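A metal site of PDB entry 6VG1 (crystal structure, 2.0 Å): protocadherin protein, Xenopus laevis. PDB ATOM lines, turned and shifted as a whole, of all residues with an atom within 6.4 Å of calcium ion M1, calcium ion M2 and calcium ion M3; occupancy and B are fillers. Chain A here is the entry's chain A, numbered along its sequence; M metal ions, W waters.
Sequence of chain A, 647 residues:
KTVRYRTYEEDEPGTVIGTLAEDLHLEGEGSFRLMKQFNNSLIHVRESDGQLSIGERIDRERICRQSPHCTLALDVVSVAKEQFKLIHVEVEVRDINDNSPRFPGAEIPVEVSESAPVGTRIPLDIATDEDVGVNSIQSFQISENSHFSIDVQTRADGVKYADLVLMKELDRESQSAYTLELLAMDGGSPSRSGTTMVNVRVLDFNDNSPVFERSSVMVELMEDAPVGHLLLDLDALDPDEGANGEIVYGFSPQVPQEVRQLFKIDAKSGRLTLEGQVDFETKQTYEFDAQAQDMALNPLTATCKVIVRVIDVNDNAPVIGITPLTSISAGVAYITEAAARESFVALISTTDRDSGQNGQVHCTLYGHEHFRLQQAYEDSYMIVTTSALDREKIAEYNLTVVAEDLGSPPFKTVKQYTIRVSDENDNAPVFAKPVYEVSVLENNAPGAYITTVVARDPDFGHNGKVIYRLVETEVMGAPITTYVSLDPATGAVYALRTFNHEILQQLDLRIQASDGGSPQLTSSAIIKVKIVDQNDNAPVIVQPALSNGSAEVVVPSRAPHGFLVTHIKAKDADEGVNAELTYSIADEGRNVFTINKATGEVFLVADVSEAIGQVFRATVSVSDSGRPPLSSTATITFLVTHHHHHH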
ATOM      1  N   GLU A   9      -3.499 -21.514  16.343  1.00  0.00           N
ATOM      2  CA  GLU A   9      -3.191 -20.092  16.389  1.00  0.00           C
ATOM      3  C   GLU A   9      -4.121 -19.298  15.472  1.00  0.00           C
ATOM      4  O   GLU A   9      -4.708 -19.844  14.538  1.00  0.00           O
ATOM      5  CB  GLU A   9      -1.726 -19.839  15.999  1.00  0.00           C
ATOM      6  CG  GLU A   9      -1.394 -20.093  14.547  1.00  0.00           C
ATOM      7  CD  GLU A   9      -0.055 -19.498  14.131  1.00  0.00           C
ATOM      8  OE1 GLU A   9       0.256 -18.362  14.573  1.00  0.00           O
ATOM      9  OE2 GLU A   9       0.701 -20.151  13.372  1.00  0.00           O
ATOM     10  N   GLU A  10      -4.268 -18.005  15.757  1.00  0.00           N
ATOM     11  CA  GLU A  10      -5.074 -17.098  14.949  1.00  0.00           C
ATOM     12  C   GLU A  10      -6.500 -17.627  14.756  1.00  0.00           C
ATOM     13  O   GLU A  10      -7.091 -17.480  13.687  1.00  0.00           O
ATOM     14  CB  GLU A  10      -4.428 -16.837  13.582  1.00  0.00           C
ATOM     15  CG  GLU A  10      -2.919 -16.730  13.553  1.00  0.00           C
ATOM     16  CD  GLU A  10      -2.417 -15.288  13.462  1.00  0.00           C
ATOM     17  OE1 GLU A  10      -3.181 -14.358  13.774  1.00  0.00           O
ATOM     18  OE2 GLU A  10      -1.239 -15.112  13.079  1.00  0.00           O
ATOM     19  N   ARG A  57      -6.368 -12.137  19.998  1.00  0.00           N
ATOM     20  CA  ARG A  57      -5.669 -12.788  18.898  1.00  0.00           C
ATOM     21  C   ARG A  57      -4.478 -13.574  19.416  1.00  0.00           C
ATOM     22  O   ARG A  57      -3.725 -13.094  20.274  1.00  0.00           O
ATOM     23  CB  ARG A  57      -5.230 -11.727  17.902  1.00  0.00           C
ATOM     24  CG  ARG A  57      -4.500 -12.231  16.682  1.00  0.00           C
ATOM     25  CD  ARG A  57      -4.144 -11.036  15.798  1.00  0.00           C
ATOM     26  NE  ARG A  57      -3.417 -11.404  14.589  1.00  0.00           N
ATOM     27  CZ  ARG A  57      -2.098 -11.485  14.522  1.00  0.00           C
ATOM     28  NH1 ARG A  57      -1.347 -11.234  15.581  1.00  0.00           N
ATOM     29  NH2 ARG A  57      -1.514 -11.812  13.375  1.00  0.00           N
ATOM     30  N   ILE A  58      -4.304 -14.785  18.899  1.00  0.00           N
ATOM     31  CA  ILE A  58      -3.212 -15.666  19.302  1.00  0.00           C
ATOM     32  C   ILE A  58      -2.329 -15.927  18.083  1.00  0.00           C
ATOM     33  O   ILE A  58      -2.709 -16.710  17.207  1.00  0.00           O
ATOM     34  CB  ILE A  58      -3.710 -16.987  19.893  1.00  0.00           C
ATOM     35  CG1 ILE A  58      -4.534 -16.744  21.151  1.00  0.00           C
ATOM     36  CG2 ILE A  58      -2.531 -17.911  20.184  1.00  0.00           C
ATOM     37  CD1 ILE A  58      -5.223 -17.994  21.677  1.00  0.00           C
ATOM     38  N   ASP A  59      -1.158 -15.283  18.038  1.00  0.00           N
ATOM     39  CA  ASP A  59      -0.208 -15.450  16.937  1.00  0.00           C
ATOM     40  C   ASP A  59       1.010 -16.206  17.444  1.00  0.00           C
ATOM     41  O   ASP A  59       1.836 -15.649  18.174  1.00  0.00           O
ATOM     42  CB  ASP A  59       0.190 -14.088  16.368  1.00  0.00           C
ATOM     43  CG  ASP A  59       1.049 -14.206  15.112  1.00  0.00           C
ATOM     44  OD1 ASP A  59       1.314 -15.344  14.665  1.00  0.00           O
ATOM     45  OD2 ASP A  59       1.452 -13.159  14.564  1.00  0.00           O
ATOM     46  N   ARG A  60       1.141 -17.466  17.020  1.00  0.00           N
ATOM     47  CA  ARG A  60       2.259 -18.285  17.496  1.00  0.00           C
ATOM     48  C   ARG A  60       3.597 -17.640  17.149  1.00  0.00           C
ATOM     49  O   ARG A  60       4.498 -17.570  17.986  1.00  0.00           O
ATOM     50  CB  ARG A  60       2.177 -19.688  16.903  1.00  0.00           C
ATOM     51  CG  ARG A  60       2.954 -20.730  17.702  1.00  0.00           C
ATOM     52  CD  ARG A  60       3.479 -21.851  16.838  1.00  0.00           C
ATOM     53  NE  ARG A  60       4.258 -21.331  15.710  1.00  0.00           N
ATOM     54  CZ  ARG A  60       5.438 -20.727  15.823  1.00  0.00           C
ATOM     55  NH1 ARG A  60       5.978 -20.563  17.022  1.00  0.00           N
ATOM     56  NH2 ARG A  60       6.067 -20.299  14.746  1.00  0.00           N
ATOM     57  N   GLU A  61       3.746 -17.173  15.914  1.00  0.00           N
ATOM     58  CA  GLU A  61       5.010 -16.596  15.475  1.00  0.00           C
ATOM     59  C   GLU A  61       5.401 -15.353  16.276  1.00  0.00           C
ATOM     60  O   GLU A  61       6.566 -14.940  16.206  1.00  0.00           O
ATOM     61  CB  GLU A  61       4.937 -16.264  13.984  1.00  0.00           C
ATOM     62  CG  GLU A  61       5.074 -17.477  13.043  1.00  0.00           C
ATOM     63  CD  GLU A  61       3.781 -18.233  12.822  1.00  0.00           C
ATOM     64  OE1 GLU A  61       2.738 -17.603  12.545  1.00  0.00           O
ATOM     65  OE2 GLU A  61       3.805 -19.475  12.915  1.00  0.00           O
ATOM     66  N   ARG A  62       4.480 -14.766  17.044  1.00  0.00           N
ATOM     67  CA  ARG A  62       4.778 -13.595  17.855  1.00  0.00           C
ATOM     68  C   ARG A  62       5.104 -13.936  19.299  1.00  0.00           C
ATOM     69  O   ARG A  62       5.817 -13.173  19.955  1.00  0.00           O
ATOM     70  CB  ARG A  62       3.610 -12.610  17.829  1.00  0.00           C
ATOM     71  CG  ARG A  62       3.804 -11.406  18.736  1.00  0.00           C
ATOM     72  CD  ARG A  62       2.655 -10.404  18.604  1.00  0.00           C
ATOM     73  NE  ARG A  62       1.368 -10.996  18.970  1.00  0.00           N
ATOM     74  CZ  ARG A  62       0.921 -11.117  20.214  1.00  0.00           C
ATOM     75  NH1 ARG A  62       1.664 -10.704  21.231  1.00  0.00           N
ATOM     76  NH2 ARG A  62      -0.261 -11.665  20.443  1.00  0.00           N
ATOM     77  N   ASP A  95       0.662 -24.849  15.194  1.00  0.00           N
ATOM     78  CA  ASP A  95       1.162 -23.915  14.194  1.00  0.00           C
ATOM     79  C   ASP A  95       0.322 -24.009  12.921  1.00  0.00           C
ATOM     80  O   ASP A  95      -0.049 -25.101  12.486  1.00  0.00           O
ATOM     81  CB  ASP A  95       2.627 -24.195  13.874  1.00  0.00           C
ATOM     82  CG  ASP A  95       3.173 -23.302  12.770  1.00  0.00           C
ATOM     83  OD1 ASP A  95       2.477 -22.354  12.340  1.00  0.00           O
ATOM     84  OD2 ASP A  95       4.314 -23.546  12.316  1.00  0.00           O
ATOM     85  N   ILE A  96       0.051 -22.839  12.326  1.00  0.00           N
ATOM     86  CA  ILE A  96      -0.629 -22.735  11.044  1.00  0.00           C
ATOM     87  C   ILE A  96       0.363 -22.181  10.041  1.00  0.00           C
ATOM     88  O   ILE A  96       1.307 -21.470  10.406  1.00  0.00           O
ATOM     89  CB  ILE A  96      -1.892 -21.866  11.151  1.00  0.00           C
ATOM     90  CG1 ILE A  96      -2.889 -22.234  10.052  1.00  0.00           C
ATOM     91  CG2 ILE A  96      -1.554 -20.391  11.051  1.00  0.00           C
ATOM     92  CD1 ILE A  96      -3.472 -23.634  10.197  1.00  0.00           C
ATOM     93  N   ASN A  97       0.144 -22.508   8.767  1.00  0.00           N
ATOM     94  CA  ASN A  97       1.085 -22.160   7.700  1.00  0.00           C
ATOM     95  C   ASN A  97       0.755 -20.795   7.086  1.00  0.00           C
ATOM     96  O   ASN A  97       0.609 -20.643   5.875  1.00  0.00           O
ATOM     97  CB  ASN A  97       1.053 -23.257   6.647  1.00  0.00           C
ATOM     98  CG  ASN A  97       2.206 -23.146   5.660  1.00  0.00           C
ATOM     99  OD1 ASN A  97       3.279 -22.637   5.998  1.00  0.00           O
ATOM    100  ND2 ASN A  97       1.984 -23.613   4.440  1.00  0.00           N
ATOM    101  N   ASP A  98       0.648 -19.793   7.952  1.00  0.00           N
ATOM    102  CA  ASP A  98       0.315 -18.435   7.538  1.00  0.00           C
ATOM    103  C   ASP A  98       1.545 -17.602   7.232  1.00  0.00           C
ATOM    104  O   ASP A  98       1.452 -16.377   7.183  1.00  0.00           O
ATOM    105  CB  ASP A  98      -0.528 -17.742   8.620  1.00  0.00           C
ATOM    106  CG  ASP A  98       0.083 -17.859  10.017  1.00  0.00           C
ATOM    107  OD1 ASP A  98       1.127 -18.532  10.182  1.00  0.00           O
ATOM    108  OD2 ASP A  98      -0.508 -17.281  10.954  1.00  0.00           O
ATOM    109  N   ASN A  99       2.689 -18.242   7.006  1.00  0.00           N
ATOM    110  CA  ASN A  99       3.893 -17.532   6.608  1.00  0.00           C
ATOM    111  C   ASN A  99       4.591 -18.317   5.520  1.00  0.00           C
ATOM    112  O   ASN A  99       4.736 -19.549   5.615  1.00  0.00           O
ATOM    113  CB  ASN A  99       4.840 -17.308   7.786  1.00  0.00           C
ATOM    114  CG  ASN A  99       4.414 -16.148   8.658  1.00  0.00           C
ATOM    115  OD1 ASN A  99       4.352 -15.003   8.194  1.00  0.00           O
ATOM    116  ND2 ASN A  99       4.099 -16.418   9.911  1.00  0.00           N
ATOM    117  N   SER A 100       5.048 -17.586   4.491  1.00  0.00           N
ATOM    118  CA  SER A 100       5.681 -18.149   3.332  1.00  0.00           C
ATOM    119  C   SER A 100       7.167 -17.853   3.344  1.00  0.00           C
ATOM    120  O   SER A 100       7.602 -16.842   3.900  1.00  0.00           O
ATOM    121  CB  SER A 100       5.049 -17.556   2.086  1.00  0.00           C
ATOM    122  OG  SER A 100       4.871 -16.149   2.252  1.00  0.00           O
ATOM    123  N   PRO A 101       7.966 -18.693   2.700  1.00  0.00           N
ATOM    124  CA  PRO A 101       9.413 -18.410   2.620  1.00  0.00           C
ATOM    125  C   PRO A 101       9.669 -17.050   2.000  1.00  0.00           C
ATOM    126  O   PRO A 101       9.007 -16.647   1.045  1.00  0.00           O
ATOM    127  CB  PRO A 101       9.954 -19.549   1.756  1.00  0.00           C
ATOM    128  CG  PRO A 101       8.962 -20.669   1.923  1.00  0.00           C
ATOM    129  CD  PRO A 101       7.608 -19.982   2.074  1.00  0.00           C
ATOM    130  N   ASP A 129      11.310 -18.784   6.759  1.00  0.00           N
ATOM    131  CA  ASP A 129       9.882 -19.060   6.908  1.00  0.00           C
ATOM    132  C   ASP A 129       9.592 -19.038   8.396  1.00  0.00           C
ATOM    133  O   ASP A 129      10.138 -19.860   9.143  1.00  0.00           O
ATOM    134  CB  ASP A 129       9.512 -20.410   6.298  1.00  0.00           C
ATOM    135  CG  ASP A 129       8.005 -20.659   6.278  1.00  0.00           C
ATOM    136  OD1 ASP A 129       7.208 -19.923   6.915  1.00  0.00           O
ATOM    137  OD2 ASP A 129       7.613 -21.655   5.623  1.00  0.00           O
ATOM    138  N   GLU A 130       8.759 -18.093   8.837  1.00  0.00           N
ATOM    139  CA  GLU A 130       8.559 -17.880  10.263  1.00  0.00           C
ATOM    140  C   GLU A 130       7.695 -18.958  10.920  1.00  0.00           C
ATOM    141  O   GLU A 130       7.508 -18.888  12.137  1.00  0.00           O
ATOM    142  CB  GLU A 130       7.942 -16.494  10.495  1.00  0.00           C
ATOM    143  CG  GLU A 130       8.898 -15.358  10.171  1.00  0.00           C
ATOM    144  CD  GLU A 130       8.389 -14.011  10.652  1.00  0.00           C
ATOM    145  OE1 GLU A 130       7.215 -13.940  11.079  1.00  0.00           O
ATOM    146  OE2 GLU A 130       9.159 -13.030  10.600  1.00  0.00           O
ATOM    147  N   ASP A 131       7.171 -19.914  10.166  1.00  0.00           N
ATOM    148  CA  ASP A 131       6.516 -21.073  10.767  1.00  0.00           C
ATOM    149  C   ASP A 131       7.573 -22.041  11.288  1.00  0.00           C
ATOM    150  O   ASP A 131       8.781 -21.759  11.237  1.00  0.00           O
ATOM    151  CB  ASP A 131       5.598 -21.727   9.741  1.00  0.00           C
ATOM    152  CG  ASP A 131       4.607 -20.743   9.129  1.00  0.00           C
ATOM    153  OD1 ASP A 131       4.065 -19.870   9.859  1.00  0.00           O
ATOM    154  OD2 ASP A 131       4.367 -20.836   7.896  1.00  0.00           O
ATOM    155  N   VAL A 132       7.135 -23.191  11.811  1.00  0.00           N
ATOM    156  CA  VAL A 132       8.061 -24.195  12.319  1.00  0.00           C
ATOM    157  C   VAL A 132       7.693 -25.559  11.735  1.00  0.00           C
ATOM    158  O   VAL A 132       6.657 -25.722  11.093  1.00  0.00           O
ATOM    159  CB  VAL A 132       8.064 -24.260  13.874  1.00  0.00           C
ATOM    160  CG1 VAL A 132       8.549 -22.950  14.472  1.00  0.00           C
ATOM    161  CG2 VAL A 132       6.678 -24.611  14.385  1.00  0.00           C
ATOM    162  N   VAL A 134       7.162 -28.823   9.620  1.00  0.00           N
ATOM    163  CA  VAL A 134       6.959 -28.977   8.183  1.00  0.00           C
ATOM    164  C   VAL A 134       6.637 -27.638   7.544  1.00  0.00           C
ATOM    165  O   VAL A 134       6.967 -27.390   6.378  1.00  0.00           O
ATOM    166  CB  VAL A 134       5.859 -30.009   7.889  1.00  0.00           C
ATOM    167  CG1 VAL A 134       6.189 -31.335   8.545  1.00  0.00           C
ATOM    168  CG2 VAL A 134       4.497 -29.476   8.335  1.00  0.00           C
ATOM    169  N   ASN A 135       5.975 -26.746   8.287  1.00  0.00           N
ATOM    170  CA  ASN A 135       5.647 -25.423   7.765  1.00  0.00           C
ATOM    171  C   ASN A 135       6.870 -24.540   7.586  1.00  0.00           C
ATOM    172  O   ASN A 135       6.733 -23.413   7.099  1.00  0.00           O
ATOM    173  CB  ASN A 135       4.639 -24.737   8.672  1.00  0.00           C
ATOM    174  CG  ASN A 135       3.290 -25.422   8.651  1.00  0.00           C
ATOM    175  OD1 ASN A 135       3.066 -26.316   7.835  1.00  0.00           O
ATOM    176  ND2 ASN A 135       2.395 -25.003   9.534  1.00  0.00           N
ATOM    177  N   SER A 136       8.049 -25.030   7.950  1.00  0.00           N
ATOM    178  CA  SER A 136       9.301 -24.314   7.728  1.00  0.00           C
ATOM    179  C   SER A 136       9.858 -24.678   6.351  1.00  0.00           C
ATOM    180  O   SER A 136       9.326 -25.547   5.642  1.00  0.00           O
ATOM    181  CB  SER A 136      10.306 -24.643   8.813  1.00  0.00           C
ATOM    182  OG  SER A 136      10.808 -25.968   8.649  1.00  0.00           O
ATOM    183  N   ILE A 137      10.950 -24.035   5.966  1.00  0.00           N
ATOM    184  CA  ILE A 137      11.559 -24.275   4.657  1.00  0.00           C
ATOM    185  C   ILE A 137      12.099 -25.697   4.620  1.00  0.00           C
ATOM    186  O   ILE A 137      12.954 -26.074   5.428  1.00  0.00           O
ATOM    187  CB  ILE A 137      12.666 -23.256   4.380  1.00  0.00           C
ATOM    188  CG1 ILE A 137      12.049 -21.861   4.233  1.00  0.00           C
ATOM    189  CG2 ILE A 137      13.442 -23.630   3.118  1.00  0.00           C
ATOM    190  CD1 ILE A 137      13.070 -20.732   4.124  1.00  0.00           C
ATOM    191  N   ASP A 186       8.067 -24.877   1.585  1.00  0.00           N
ATOM    192  CA  ASP A 186       7.838 -25.577   2.838  1.00  0.00           C
ATOM    193  C   ASP A 186       6.959 -26.811   2.618  1.00  0.00           C
ATOM    194  O   ASP A 186       6.495 -27.093   1.508  1.00  0.00           O
ATOM    195  CB  ASP A 186       7.202 -24.626   3.866  1.00  0.00           C
ATOM    196  CG  ASP A 186       5.848 -24.059   3.405  1.00  0.00           C
ATOM    197  OD1 ASP A 186       5.137 -24.727   2.616  1.00  0.00           O
ATOM    198  OD2 ASP A 186       5.499 -22.941   3.840  1.00  0.00           O
ATOM    199  N   GLY A 187       6.703 -27.535   3.715  1.00  0.00           N
ATOM    200  CA  GLY A 187       5.969 -28.781   3.652  1.00  0.00           C
ATOM    201  C   GLY A 187       4.462 -28.601   3.792  1.00  0.00           C
ATOM    202  O   GLY A 187       3.949 -27.490   3.974  1.00  0.00           O
ATOM    203  N   ARG A 192       3.812 -23.166   0.275  1.00  0.00           N
ATOM    204  CA  ARG A 192       4.099 -21.770  -0.016  1.00  0.00           C
ATOM    205  C   ARG A 192       5.554 -21.636  -0.442  1.00  0.00           C
ATOM    206  O   ARG A 192       6.461 -22.112   0.255  1.00  0.00           O
ATOM    207  CB  ARG A 192       3.790 -20.887   1.186  1.00  0.00           C
ATOM    208  CG  ARG A 192       2.288 -20.843   1.493  1.00  0.00           C
ATOM    209  CD  ARG A 192       1.979 -20.398   2.914  1.00  0.00           C
ATOM    210  NE  ARG A 192       2.087 -18.958   3.118  1.00  0.00           N
ATOM    211  CZ  ARG A 192       1.051 -18.138   3.240  1.00  0.00           C
ATOM    212  NH1 ARG A 192      -0.184 -18.604   3.180  1.00  0.00           N
ATOM    213  NH2 ARG A 192       1.257 -16.840   3.439  1.00  0.00           N
HETATM  214 CA    CA M   1       0.595 -16.725  12.832  1.00  0.00          CA
HETATM  215 CA    CA M   2       2.294 -20.116  11.528  1.00  0.00          CA
HETATM  216 CA    CA M   3       5.460 -21.747   6.077  1.00  0.00          CA
HETATM  217  O   HOH W   1       1.297 -14.085  11.753  1.00  0.00           O
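The nearest printed residue that does not touch calcium ion M1 is Arg 60 (4.3 Å).
Six residues have an atom within 4 Å of calcium ion M3: Asn 97, Asn 99, Asp 129, Asp 131, Asn 135 and Asp 186.
The side-chain carboxylate (OD2) of Asp 129 is bound to calcium ion M3, at 2.2 Å. Calcium ion M3 is bound by OD2 of Asp 131. O of Asn 135 is bound to calcium ion M3. Calcium ion M3 is bound by OD1 of Asn 97, 2.4 Å away. The backbone carbonyl oxygen (O) of Asn 99 binds calcium ion M3 (2.4 Å). OD2 of Asp 186 is bound to calcium ion M3 (2.5 Å). OD1 of Asp 129 is bound to calcium ion M3, at 2.7 Å.
The side-chain carboxylate (OE1) of Glu 61 lies close to the side-chain amide nitrogen (ND2) of Asn 99 (3.2 Å). OE2 of Glu 61 sits close to NH2 of Arg 60 (3.0 Å). The guanidinium group (NE) of Arg 60 sits close to the side-chain carboxylate (OD1) of Asp 95 (3.9 Å). N of Val 132 is in hydrogen-bond range of OD2 of Asp 95 (2.9 Å). The side-chain carboxylate (OD2) of Asp 59 lies within salt-bridge range of the guanidinium group (NH2) of Arg 57. The guanidinium group (NH2) of Arg 57 lies within salt-bridge range of the side-chain carboxylate (OE1) of Glu 10 (3.1 Å). The backbone NH of Glu 10 lies within hydrogen-bond range of the backbone carbonyl oxygen of Ile 58 (2.5 Å). The backbone NH (N) of Arg 192 lies within hydrogen-bond range of the side-chain carboxylate (OD1) of Asp 186, 3.1 Å away.
Calcium ion M2 is bound by the backbone carbonyl oxygen (O) of Ile 96 (2.0 Å), the side-chain carboxylate (OE2) of Glu 61 (2.1 Å), the side-chain carboxylate (OD1) of Asp 98 (2.4 Å), the side-chain carboxylate (OD1) of Asp 95 (2.4 Å), the side-chain carboxylate (OE2) of Glu 9 (2.4 Å), the side-chain carboxylate (OD1) of Asp 131 (2.4 Å) and the side-chain carboxylate (OE1) of Glu 61 (2.7 Å).
Six residues have an atom within 4 Å of calcium ion M2: Glu 9, Glu 61, Asp 95, Ile 96, Asp 98 and Asp 131.
Calcium ion M1 is bound by the side-chain carboxylate of Asp 98 (2.2 Å), the side-chain carboxylate of Glu 61 (2.3 Å), the side-chain carboxylate of Asp 59 (2.4 Å), the side-chain carboxylate of Glu 9 (2.4 Å) and the side-chain carboxylate of Glu 10 (2.5 Å). Slightly farther from calcium ion M1 lies water W1 (2.9 Å).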
